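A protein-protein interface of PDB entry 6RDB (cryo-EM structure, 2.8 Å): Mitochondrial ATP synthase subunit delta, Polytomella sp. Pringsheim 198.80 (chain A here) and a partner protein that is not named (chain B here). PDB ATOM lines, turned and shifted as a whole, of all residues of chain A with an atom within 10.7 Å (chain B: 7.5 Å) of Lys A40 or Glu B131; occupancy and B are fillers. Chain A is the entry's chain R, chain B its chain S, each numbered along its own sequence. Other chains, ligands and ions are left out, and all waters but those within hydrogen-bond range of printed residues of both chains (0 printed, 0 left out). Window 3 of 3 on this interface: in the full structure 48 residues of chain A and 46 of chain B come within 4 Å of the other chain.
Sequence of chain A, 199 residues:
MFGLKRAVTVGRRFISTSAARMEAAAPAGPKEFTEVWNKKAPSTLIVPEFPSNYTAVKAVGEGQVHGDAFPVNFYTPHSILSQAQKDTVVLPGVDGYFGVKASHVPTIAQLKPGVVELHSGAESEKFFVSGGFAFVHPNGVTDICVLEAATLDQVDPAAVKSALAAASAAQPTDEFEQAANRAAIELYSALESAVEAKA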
ATOM      1  N   GLU A  32     -18.615 -26.659  28.624  1.00  0.00           N
ATOM      2  CA  GLU A  32     -18.120 -28.027  28.524  1.00  0.00           C
ATOM      3  C   GLU A  32     -16.630 -28.106  28.828  1.00  0.00           C
ATOM      4  O   GLU A  32     -16.149 -29.144  29.295  1.00  0.00           O
ATOM      5  CB  GLU A  32     -18.435 -28.584  27.133  1.00  0.00           C
ATOM      6  CG  GLU A  32     -18.118 -30.064  26.913  1.00  0.00           C
ATOM      7  CD  GLU A  32     -16.709 -30.291  26.396  1.00  0.00           C
ATOM      8  OE1 GLU A  32     -16.232 -31.442  26.429  1.00  0.00           O
ATOM      9  OE2 GLU A  32     -16.072 -29.307  25.973  1.00  0.00           O
ATOM     10  N   PHE A  33     -15.891 -27.017  28.587  1.00  0.00           N
ATOM     11  CA  PHE A  33     -14.466 -26.993  28.911  1.00  0.00           C
ATOM     12  C   PHE A  33     -14.230 -27.051  30.413  1.00  0.00           C
ATOM     13  O   PHE A  33     -13.160 -27.484  30.843  1.00  0.00           O
ATOM     14  CB  PHE A  33     -13.807 -25.744  28.317  1.00  0.00           C
ATOM     15  CG  PHE A  33     -12.294 -25.723  28.427  1.00  0.00           C
ATOM     16  CD1 PHE A  33     -11.665 -25.003  29.432  1.00  0.00           C
ATOM     17  CD2 PHE A  33     -11.506 -26.402  27.511  1.00  0.00           C
ATOM     18  CE1 PHE A  33     -10.291 -24.972  29.527  1.00  0.00           C
ATOM     19  CE2 PHE A  33     -10.124 -26.373  27.603  1.00  0.00           C
ATOM     20  CZ  PHE A  33      -9.520 -25.657  28.613  1.00  0.00           C
ATOM     21  N   THR A  34     -15.219 -26.650  31.218  1.00  0.00           N
ATOM     22  CA  THR A  34     -15.053 -26.619  32.667  1.00  0.00           C
ATOM     23  C   THR A  34     -14.943 -28.023  33.257  1.00  0.00           C
ATOM     24  O   THR A  34     -13.980 -28.324  33.971  1.00  0.00           O
ATOM     25  CB  THR A  34     -16.214 -25.862  33.313  1.00  0.00           C
ATOM     26  OG1 THR A  34     -16.415 -24.619  32.632  1.00  0.00           O
ATOM     27  CG2 THR A  34     -15.912 -25.583  34.779  1.00  0.00           C
ATOM     28  N   GLU A  35     -15.912 -28.901  32.969  1.00  0.00           N
ATOM     29  CA  GLU A  35     -15.902 -30.201  33.636  1.00  0.00           C
ATOM     30  C   GLU A  35     -14.883 -31.160  33.033  1.00  0.00           C
ATOM     31  O   GLU A  35     -14.568 -32.181  33.650  1.00  0.00           O
ATOM     32  CB  GLU A  35     -17.290 -30.857  33.632  1.00  0.00           C
ATOM     33  CG  GLU A  35     -17.758 -31.498  32.325  1.00  0.00           C
ATOM     34  CD  GLU A  35     -18.657 -30.601  31.501  1.00  0.00           C
ATOM     35  OE1 GLU A  35     -18.667 -29.382  31.745  1.00  0.00           O
ATOM     36  OE2 GLU A  35     -19.373 -31.125  30.624  1.00  0.00           O
ATOM     37  N   VAL A  36     -14.360 -30.864  31.843  1.00  0.00           N
ATOM     38  CA  VAL A  36     -13.274 -31.672  31.297  1.00  0.00           C
ATOM     39  C   VAL A  36     -11.941 -31.244  31.902  1.00  0.00           C
ATOM     40  O   VAL A  36     -11.082 -32.080  32.209  1.00  0.00           O
ATOM     41  CB  VAL A  36     -13.280 -31.583  29.760  1.00  0.00           C
ATOM     42  CG1 VAL A  36     -12.087 -32.302  29.147  1.00  0.00           C
ATOM     43  CG2 VAL A  36     -14.573 -32.163  29.225  1.00  0.00           C
ATOM     44  N   TRP A  37     -11.768 -29.938  32.131  1.00  0.00           N
ATOM     45  CA  TRP A  37     -10.548 -29.415  32.742  1.00  0.00           C
ATOM     46  C   TRP A  37     -10.413 -29.804  34.210  1.00  0.00           C
ATOM     47  O   TRP A  37      -9.299 -29.787  34.743  1.00  0.00           O
ATOM     48  CB  TRP A  37     -10.524 -27.893  32.577  1.00  0.00           C
ATOM     49  CG  TRP A  37      -9.283 -27.187  32.979  1.00  0.00           C
ATOM     50  CD1 TRP A  37      -8.192 -26.930  32.206  1.00  0.00           C
ATOM     51  CD2 TRP A  37      -9.028 -26.581  34.243  1.00  0.00           C
ATOM     52  NE1 TRP A  37      -7.254 -26.233  32.923  1.00  0.00           N
ATOM     53  CE2 TRP A  37      -7.749 -26.000  34.178  1.00  0.00           C
ATOM     54  CE3 TRP A  37      -9.755 -26.484  35.429  1.00  0.00           C
ATOM     55  CZ2 TRP A  37      -7.184 -25.336  35.249  1.00  0.00           C
ATOM     56  CZ3 TRP A  37      -9.194 -25.830  36.487  1.00  0.00           C
ATOM     57  CH2 TRP A  37      -7.921 -25.264  36.394  1.00  0.00           C
ATOM     58  N   ASN A  38     -11.510 -30.182  34.865  1.00  0.00           N
ATOM     59  CA  ASN A  38     -11.463 -30.656  36.241  1.00  0.00           C
ATOM     60  C   ASN A  38     -10.977 -32.096  36.359  1.00  0.00           C
ATOM     61  O   ASN A  38     -10.848 -32.595  37.481  1.00  0.00           O
ATOM     62  CB  ASN A  38     -12.843 -30.535  36.887  1.00  0.00           C
ATOM     63  CG  ASN A  38     -13.301 -29.100  37.019  1.00  0.00           C
ATOM     64  OD1 ASN A  38     -14.476 -28.791  36.821  1.00  0.00           O
ATOM     65  ND2 ASN A  38     -12.376 -28.213  37.356  1.00  0.00           N
ATOM     66  N   LYS A  39     -10.705 -32.770  35.240  1.00  0.00           N
ATOM     67  CA  LYS A  39     -10.232 -34.147  35.254  1.00  0.00           C
ATOM     68  C   LYS A  39      -8.798 -34.317  34.783  1.00  0.00           C
ATOM     69  O   LYS A  39      -8.262 -35.425  34.900  1.00  0.00           O
ATOM     70  CB  LYS A  39     -11.138 -35.046  34.393  1.00  0.00           C
ATOM     71  CG  LYS A  39     -12.321 -35.666  35.132  1.00  0.00           C
ATOM     72  CD  LYS A  39     -13.417 -34.667  35.427  1.00  0.00           C
ATOM     73  CE  LYS A  39     -14.612 -35.329  36.071  1.00  0.00           C
ATOM     74  NZ  LYS A  39     -15.631 -34.326  36.480  1.00  0.00           N
ATOM     75  N   LYS A  40      -8.168 -33.277  34.247  1.00  0.00           N
ATOM     76  CA  LYS A  40      -6.774 -33.348  33.823  1.00  0.00           C
ATOM     77  C   LYS A  40      -5.862 -32.404  34.589  1.00  0.00           C
ATOM     78  O   LYS A  40      -4.703 -32.739  34.838  1.00  0.00           O
ATOM     79  CB  LYS A  40      -6.665 -33.055  32.324  1.00  0.00           C
ATOM     80  CG  LYS A  40      -5.358 -33.509  31.710  1.00  0.00           C
ATOM     81  CD  LYS A  40      -5.158 -35.005  31.846  1.00  0.00           C
ATOM     82  CE  LYS A  40      -6.152 -35.781  30.999  1.00  0.00           C
ATOM     83  NZ  LYS A  40      -5.959 -35.550  29.542  1.00  0.00           N
ATOM     84  N   ALA A  41      -6.355 -31.234  34.970  1.00  0.00           N
ATOM     85  CA  ALA A  41      -5.572 -30.283  35.737  1.00  0.00           C
ATOM     86  C   ALA A  41      -5.506 -30.709  37.200  1.00  0.00           C
ATOM     87  O   ALA A  41      -6.269 -31.576  37.636  1.00  0.00           O
ATOM     88  CB  ALA A  41      -6.190 -28.893  35.617  1.00  0.00           C
ATOM     89  N   PRO A  42      -4.574 -30.146  37.976  1.00  0.00           N
ATOM     90  CA  PRO A  42      -4.672 -30.265  39.435  1.00  0.00           C
ATOM     91  C   PRO A  42      -5.939 -29.610  39.964  1.00  0.00           C
ATOM     92  O   PRO A  42      -6.484 -28.679  39.367  1.00  0.00           O
ATOM     93  CB  PRO A  42      -3.415 -29.541  39.937  1.00  0.00           C
ATOM     94  CG  PRO A  42      -2.852 -28.834  38.735  1.00  0.00           C
ATOM     95  CD  PRO A  42      -3.239 -29.674  37.577  1.00  0.00           C
ATOM     96  N   SER A  43      -6.411 -30.113  41.104  1.00  0.00           N
ATOM     97  CA  SER A  43      -7.656 -29.629  41.687  1.00  0.00           C
ATOM     98  C   SER A  43      -7.499 -28.310  42.433  1.00  0.00           C
ATOM     99  O   SER A  43      -8.507 -27.749  42.876  1.00  0.00           O
ATOM    100  CB  SER A  43      -8.240 -30.683  42.631  1.00  0.00           C
ATOM    101  OG  SER A  43      -8.608 -31.855  41.925  1.00  0.00           O
ATOM    102  N   THR A  44      -6.275 -27.804  42.582  1.00  0.00           N
ATOM    103  CA  THR A  44      -6.054 -26.574  43.332  1.00  0.00           C
ATOM    104  C   THR A  44      -6.411 -25.320  42.541  1.00  0.00           C
ATOM    105  O   THR A  44      -6.582 -24.256  43.144  1.00  0.00           O
ATOM    106  CB  THR A  44      -4.595 -26.501  43.801  1.00  0.00           C
ATOM    107  OG1 THR A  44      -4.416 -25.356  44.645  1.00  0.00           O
ATOM    108  CG2 THR A  44      -3.638 -26.418  42.616  1.00  0.00           C
ATOM    109  N   LEU A  45      -6.532 -25.417  41.219  1.00  0.00           N
ATOM    110  CA  LEU A  45      -6.736 -24.249  40.376  1.00  0.00           C
ATOM    111  C   LEU A  45      -8.195 -24.120  39.955  1.00  0.00           C
ATOM    112  O   LEU A  45      -8.829 -25.097  39.553  1.00  0.00           O
ATOM    113  CB  LEU A  45      -5.855 -24.330  39.130  1.00  0.00           C
ATOM    114  CG  LEU A  45      -4.339 -24.387  39.293  1.00  0.00           C
ATOM    115  CD1 LEU A  45      -3.692 -24.651  37.945  1.00  0.00           C
ATOM    116  CD2 LEU A  45      -3.804 -23.103  39.911  1.00  0.00           C
ATOM    117  N   VAL A  47     -11.020 -22.723  37.256  1.00  0.00           N
ATOM    118  CA  VAL A  47     -11.067 -22.807  35.789  1.00  0.00           C
ATOM    119  C   VAL A  47     -10.643 -21.469  35.190  1.00  0.00           C
ATOM    120  O   VAL A  47     -10.874 -20.415  35.815  1.00  0.00           O
ATOM    121  CB  VAL A  47     -12.481 -23.223  35.333  1.00  0.00           C
ATOM    122  CG1 VAL A  47     -13.546 -22.172  35.672  1.00  0.00           C
ATOM    123  CG2 VAL A  47     -12.538 -23.606  33.861  1.00  0.00           C
ATOM    124  N   PRO A  48      -9.927 -21.454  34.065  1.00  0.00           N
ATOM    125  CA  PRO A  48      -9.636 -20.180  33.405  1.00  0.00           C
ATOM    126  C   PRO A  48     -10.900 -19.531  32.876  1.00  0.00           C
ATOM    127  O   PRO A  48     -11.863 -20.201  32.501  1.00  0.00           O
ATOM    128  CB  PRO A  48      -8.695 -20.576  32.260  1.00  0.00           C
ATOM    129  CG  PRO A  48      -8.844 -22.046  32.121  1.00  0.00           C
ATOM    130  CD  PRO A  48      -9.107 -22.538  33.498  1.00  0.00           C
ATOM    131  N   VAL B  95     -11.620 -27.999  21.501  1.00  0.00           N
ATOM    132  CA  VAL B  95     -11.714 -28.619  20.188  1.00  0.00           C
ATOM    133  C   VAL B  95     -10.509 -29.529  19.996  1.00  0.00           C
ATOM    134  O   VAL B  95      -9.433 -29.305  20.562  1.00  0.00           O
ATOM    135  CB  VAL B  95     -11.829 -27.582  19.046  1.00  0.00           C
ATOM    136  CG1 VAL B  95     -12.981 -26.650  19.312  1.00  0.00           C
ATOM    137  CG2 VAL B  95     -10.547 -26.781  18.884  1.00  0.00           C
ATOM    138  N   ARG B 124       0.094 -25.492  31.076  1.00  0.00           N
ATOM    139  CA  ARG B 124       0.041 -26.949  31.032  1.00  0.00           C
ATOM    140  C   ARG B 124      -1.273 -27.505  31.567  1.00  0.00           C
ATOM    141  O   ARG B 124      -1.592 -28.664  31.292  1.00  0.00           O
ATOM    142  CB  ARG B 124       1.211 -27.540  31.816  1.00  0.00           C
ATOM    143  CG  ARG B 124       1.235 -27.132  33.274  1.00  0.00           C
ATOM    144  CD  ARG B 124       2.545 -27.508  33.940  1.00  0.00           C
ATOM    145  NE  ARG B 124       2.676 -28.947  34.131  1.00  0.00           N
ATOM    146  CZ  ARG B 124       2.395 -29.568  35.270  1.00  0.00           C
ATOM    147  NH1 ARG B 124       1.969 -28.869  36.312  1.00  0.00           N
ATOM    148  NH2 ARG B 124       2.536 -30.883  35.369  1.00  0.00           N
ATOM    149  N   ALA B 125      -2.032 -26.722  32.334  1.00  0.00           N
ATOM    150  CA  ALA B 125      -3.393 -27.124  32.665  1.00  0.00           C
ATOM    151  C   ALA B 125      -4.300 -27.027  31.448  1.00  0.00           C
ATOM    152  O   ALA B 125      -5.266 -27.788  31.328  1.00  0.00           O
ATOM    153  CB  ALA B 125      -3.936 -26.267  33.805  1.00  0.00           C
ATOM    154  N   THR B 126      -4.001 -26.093  30.545  1.00  0.00           N
ATOM    155  CA  THR B 126      -4.700 -25.978  29.273  1.00  0.00           C
ATOM    156  C   THR B 126      -4.053 -26.866  28.212  1.00  0.00           C
ATOM    157  O   THR B 126      -4.754 -27.437  27.366  1.00  0.00           O
ATOM    158  CB  THR B 126      -4.720 -24.498  28.857  1.00  0.00           C
ATOM    159  OG1 THR B 126      -5.546 -23.763  29.769  1.00  0.00           O
ATOM    160  CG2 THR B 126      -5.260 -24.285  27.451  1.00  0.00           C
ATOM    161  N   LEU B 127      -2.734 -27.067  28.290  1.00  0.00           N
ATOM    162  CA  LEU B 127      -2.012 -27.882  27.320  1.00  0.00           C
ATOM    163  C   LEU B 127      -1.996 -29.365  27.693  1.00  0.00           C
ATOM    164  O   LEU B 127      -1.194 -30.141  27.154  1.00  0.00           O
ATOM    165  CB  LEU B 127      -0.592 -27.347  27.149  1.00  0.00           C
ATOM    166  CG  LEU B 127       0.031 -27.460  25.764  1.00  0.00           C
ATOM    167  CD1 LEU B 127      -0.921 -26.866  24.756  1.00  0.00           C
ATOM    168  CD2 LEU B 127       1.365 -26.740  25.740  1.00  0.00           C
ATOM    169  N   ALA B 128      -2.870 -29.780  28.603  1.00  0.00           N
ATOM    170  CA  ALA B 128      -3.135 -31.189  28.835  1.00  0.00           C
ATOM    171  C   ALA B 128      -4.612 -31.527  28.799  1.00  0.00           C
ATOM    172  O   ALA B 128      -4.952 -32.690  28.555  1.00  0.00           O
ATOM    173  CB  ALA B 128      -2.548 -31.640  30.181  1.00  0.00           C
ATOM    174  N   THR B 129      -5.498 -30.553  29.016  1.00  0.00           N
ATOM    175  CA  THR B 129      -6.926 -30.779  28.824  1.00  0.00           C
ATOM    176  C   THR B 129      -7.271 -30.954  27.356  1.00  0.00           C
ATOM    177  O   THR B 129      -7.932 -31.927  26.978  1.00  0.00           O
ATOM    178  CB  THR B 129      -7.711 -29.617  29.413  1.00  0.00           C
ATOM    179  OG1 THR B 129      -7.312 -29.440  30.773  1.00  0.00           O
ATOM    180  CG2 THR B 129      -9.195 -29.882  29.325  1.00  0.00           C
ATOM    181  N   THR B 130      -6.826 -30.026  26.513  1.00  0.00           N
ATOM    182  CA  THR B 130      -7.077 -30.106  25.084  1.00  0.00           C
ATOM    183  C   THR B 130      -6.198 -31.135  24.386  1.00  0.00           C
ATOM    184  O   THR B 130      -6.444 -31.442  23.215  1.00  0.00           O
ATOM    185  CB  THR B 130      -6.879 -28.730  24.450  1.00  0.00           C
ATOM    186  OG1 THR B 130      -5.539 -28.281  24.684  1.00  0.00           O
ATOM    187  CG2 THR B 130      -7.849 -27.735  25.058  1.00  0.00           C
ATOM    188  N   GLU B 131      -5.185 -31.667  25.067  1.00  0.00           N
ATOM    189  CA  GLU B 131      -4.449 -32.810  24.548  1.00  0.00           C
ATOM    190  C   GLU B 131      -5.313 -34.058  24.639  1.00  0.00           C
ATOM    191  O   GLU B 131      -5.526 -34.597  25.732  1.00  0.00           O
ATOM    192  CB  GLU B 131      -3.134 -33.001  25.307  1.00  0.00           C
ATOM    193  CG  GLU B 131      -2.345 -34.222  24.875  1.00  0.00           C
ATOM    194  CD  GLU B 131      -1.870 -34.157  23.436  1.00  0.00           C
ATOM    195  OE1 GLU B 131      -1.627 -33.052  22.902  1.00  0.00           O
ATOM    196  OE2 GLU B 131      -1.741 -35.239  22.836  1.00  0.00           O
ATOM    197  N   SER B 132      -5.831 -34.512  23.500  1.00  0.00           N
ATOM    198  CA  SER B 132      -6.761 -35.633  23.483  1.00  0.00           C
ATOM    199  C   SER B 132      -6.463 -36.702  22.439  1.00  0.00           C
ATOM    200  O   SER B 132      -6.876 -37.850  22.639  1.00  0.00           O
ATOM    201  CB  SER B 132      -8.192 -35.127  23.272  1.00  0.00           C
ATOM    202  OG  SER B 132      -8.587 -34.299  24.355  1.00  0.00           O
ATOM    203  N   GLU B 133      -5.763 -36.385  21.344  1.00  0.00           N
ATOM    204  CA  GLU B 133      -5.542 -37.391  20.310  1.00  0.00           C
ATOM    205  C   GLU B 133      -4.120 -37.368  19.753  1.00  0.00           C
ATOM    206  O   GLU B 133      -3.867 -37.974  18.704  1.00  0.00           O
ATOM    207  CB  GLU B 133      -6.559 -37.219  19.166  1.00  0.00           C
ATOM    208  CG  GLU B 133      -6.363 -35.975  18.295  1.00  0.00           C
ATOM    209  CD  GLU B 133      -7.047 -34.734  18.832  1.00  0.00           C
ATOM    210  OE1 GLU B 133      -7.476 -34.728  20.004  1.00  0.00           O
ATOM    211  OE2 GLU B 133      -7.140 -33.752  18.072  1.00  0.00           O
ATOM    212  N   GLY B 134      -3.173 -36.743  20.446  1.00  0.00           N
ATOM    213  CA  GLY B 134      -1.859 -36.531  19.871  1.00  0.00           C
ATOM    214  C   GLY B 134      -1.814 -35.285  19.014  1.00  0.00           C
ATOM    215  O   GLY B 134      -1.540 -35.352  17.812  1.00  0.00           O
ATOM    216  N   LYS B 135      -2.082 -34.138  19.635  1.00  0.00           N
ATOM    217  CA  LYS B 135      -2.187 -32.861  18.945  1.00  0.00           C
ATOM    218  C   LYS B 135      -0.822 -32.197  18.810  1.00  0.00           C
ATOM    219  O   LYS B 135      -0.070 -32.099  19.784  1.00  0.00           O
ATOM    220  CB  LYS B 135      -3.138 -31.939  19.712  1.00  0.00           C
ATOM    221  CG  LYS B 135      -3.033 -30.463  19.361  1.00  0.00           C
ATOM    222  CD  LYS B 135      -3.777 -29.603  20.366  1.00  0.00           C
ATOM    223  CE  LYS B 135      -5.273 -29.847  20.309  1.00  0.00           C
ATOM    224  NZ  LYS B 135      -6.024 -28.820  21.078  1.00  0.00           N
ATOM    225  N   ASP B 136      -0.507 -31.742  17.599  1.00  0.00           N
ATOM    226  CA  ASP B 136       0.679 -30.925  17.386  1.00  0.00           C
ATOM    227  C   ASP B 136       0.472 -29.564  18.038  1.00  0.00           C
ATOM    228  O   ASP B 136      -0.554 -28.910  17.824  1.00  0.00           O
ATOM    229  CB  ASP B 136       0.963 -30.767  15.892  1.00  0.00           C
ATOM    230  CG  ASP B 136       2.410 -30.388  15.599  1.00  0.00           C
ATOM    231  OD1 ASP B 136       2.886 -29.350  16.103  1.00  0.00           O
ATOM    232  OD2 ASP B 136       3.074 -31.130  14.848  1.00  0.00           O
ATOM    233  N   VAL B 137       1.447 -29.138  18.834  1.00  0.00           N
ATOM    234  CA  VAL B 137       1.348 -27.923  19.631  1.00  0.00           C
ATOM    235  C   VAL B 137       2.610 -27.104  19.405  1.00  0.00           C
ATOM    236  O   VAL B 137       3.716 -27.648  19.433  1.00  0.00           O
ATOM    237  CB  VAL B 137       1.154 -28.257  21.125  1.00  0.00           C
ATOM    238  CG1 VAL B 137       1.587 -27.119  22.018  1.00  0.00           C
ATOM    239  CG2 VAL B 137      -0.295 -28.613  21.405  1.00  0.00           C
ATOM    240  N   ARG B 157       8.113 -28.723  22.227  1.00  0.00           N
ATOM    241  CA  ARG B 157       7.082 -28.152  21.371  1.00  0.00           C
ATOM    242  C   ARG B 157       7.038 -26.635  21.484  1.00  0.00           C
ATOM    243  O   ARG B 157       6.013 -26.022  21.181  1.00  0.00           O
ATOM    244  CB  ARG B 157       5.719 -28.747  21.708  1.00  0.00           C
ATOM    245  CG  ARG B 157       5.607 -30.244  21.525  1.00  0.00           C
ATOM    246  CD  ARG B 157       4.219 -30.729  21.925  1.00  0.00           C
ATOM    247  NE  ARG B 157       3.822 -30.248  23.246  1.00  0.00           N
ATOM    248  CZ  ARG B 157       2.633 -30.477  23.796  1.00  0.00           C
ATOM    249  NH1 ARG B 157       2.354 -30.002  25.003  1.00  0.00           N
ATOM    250  NH2 ARG B 157       1.724 -31.186  23.143  1.00  0.00           N
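O of Ala B125 is in hydrogen-bond range of OG1 of Thr B129, 2.7 Å away.
OG1 of Thr B130 is in hydrogen-bond range of O of Thr B126 (2.9 Å).
The side-chain amino group of Lys B135 sits at hydrogen-bond distance from the backbone carbonyl oxygen of Thr B130 (3.4 Å).
The side-chain carboxylate of Glu B131 sits at hydrogen-bond distance from the backbone NH of Gly B134.
OE2 of Glu B131 is in hydrogen-bond range of N of Lys B135 (3.4 Å).
The side-chain carboxylate (OE1) of Glu B131 is in salt-bridge range of the guanidinium group (NH2) of Arg B157 (3.8 Å).
The indole nitrogen (NE1) of Trp A37 sits at hydrogen-bond distance from the backbone carbonyl oxygen (O) of Ala B125, 3.0 Å away.
The side-chain amino group of Lys A40 lies within hydrogen-bond range of the backbone carbonyl oxygen of Ala B128 (3.2 Å).
CE2 of Phe A33 touches CG2 of Thr B130, at 3.7 Å.
Val A36 touches Thr B129.
Thr B129 touches Trp A37 (OG1 to CD1, 3.0 Å).
CB of Lys A40 touches OG1 of Thr B129, 3.99 Å away.
NZ of Lys A40 touches O of Glu B131, 3.95 Å away.
CB of Ala B125 touches CB of Ala A41, at 3.9 Å.
Of the 16 printed residues of chain B, 5 touch a printed residue of chain A.
Hydrophobic or aromatic side chains of chain B within 4 Å of the printed part of chain A: Ala B125 and Ala B128.
Hydrophobic or aromatic side chains of chain A within 4 Å of the printed part of chain B: Phe A33, Val A36, Trp A37 and Ala A41.
Among the printed residues, no Asp or Glu carboxylate lies within 4 Å of a Lys or Arg side-chain nitrogen of the other chain.
Of the printed residues of chain B, Phe A33 touches Thr B130 (3.7 Å).
Of the printed residues of chain B, Trp A37 touches Ala B125 (3.0 Å) and Thr B129 (3.0 Å).
Of the printed residues of chain B, Lys A40 touches Ala B128 (3.2 Å), Thr B129 (3.99 Å) and Glu B131 (3.95 Å).
Printed residues of chain B within 4 Å of Ala A41: Ala B125 (3.9 Å).
Ser A43 touches none of the printed residues of chain B.
Printed residues of chain A within 4 Å of Ala B125: Trp A37 and Ala A41.
Of the printed residues of chain A, Thr B129 touches Val A36, Trp A37 and Lys A40.
Thr B130 touches one residue of chain A.
Glu B131 touches just one residue of chain A: Lys A40 (3.95 Å).
No residue of chain A comes within 4 Å of Ser B132.
No residue of chain A comes within 4 Å of Gly B134.
No residue of chain A comes within 4 Å of Lys B135.
Arg B157 touches none of the printed residues of chain A.
The nearest residue of chain A that does not touch Glu B131 is Phe A33 (7.7 Å).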
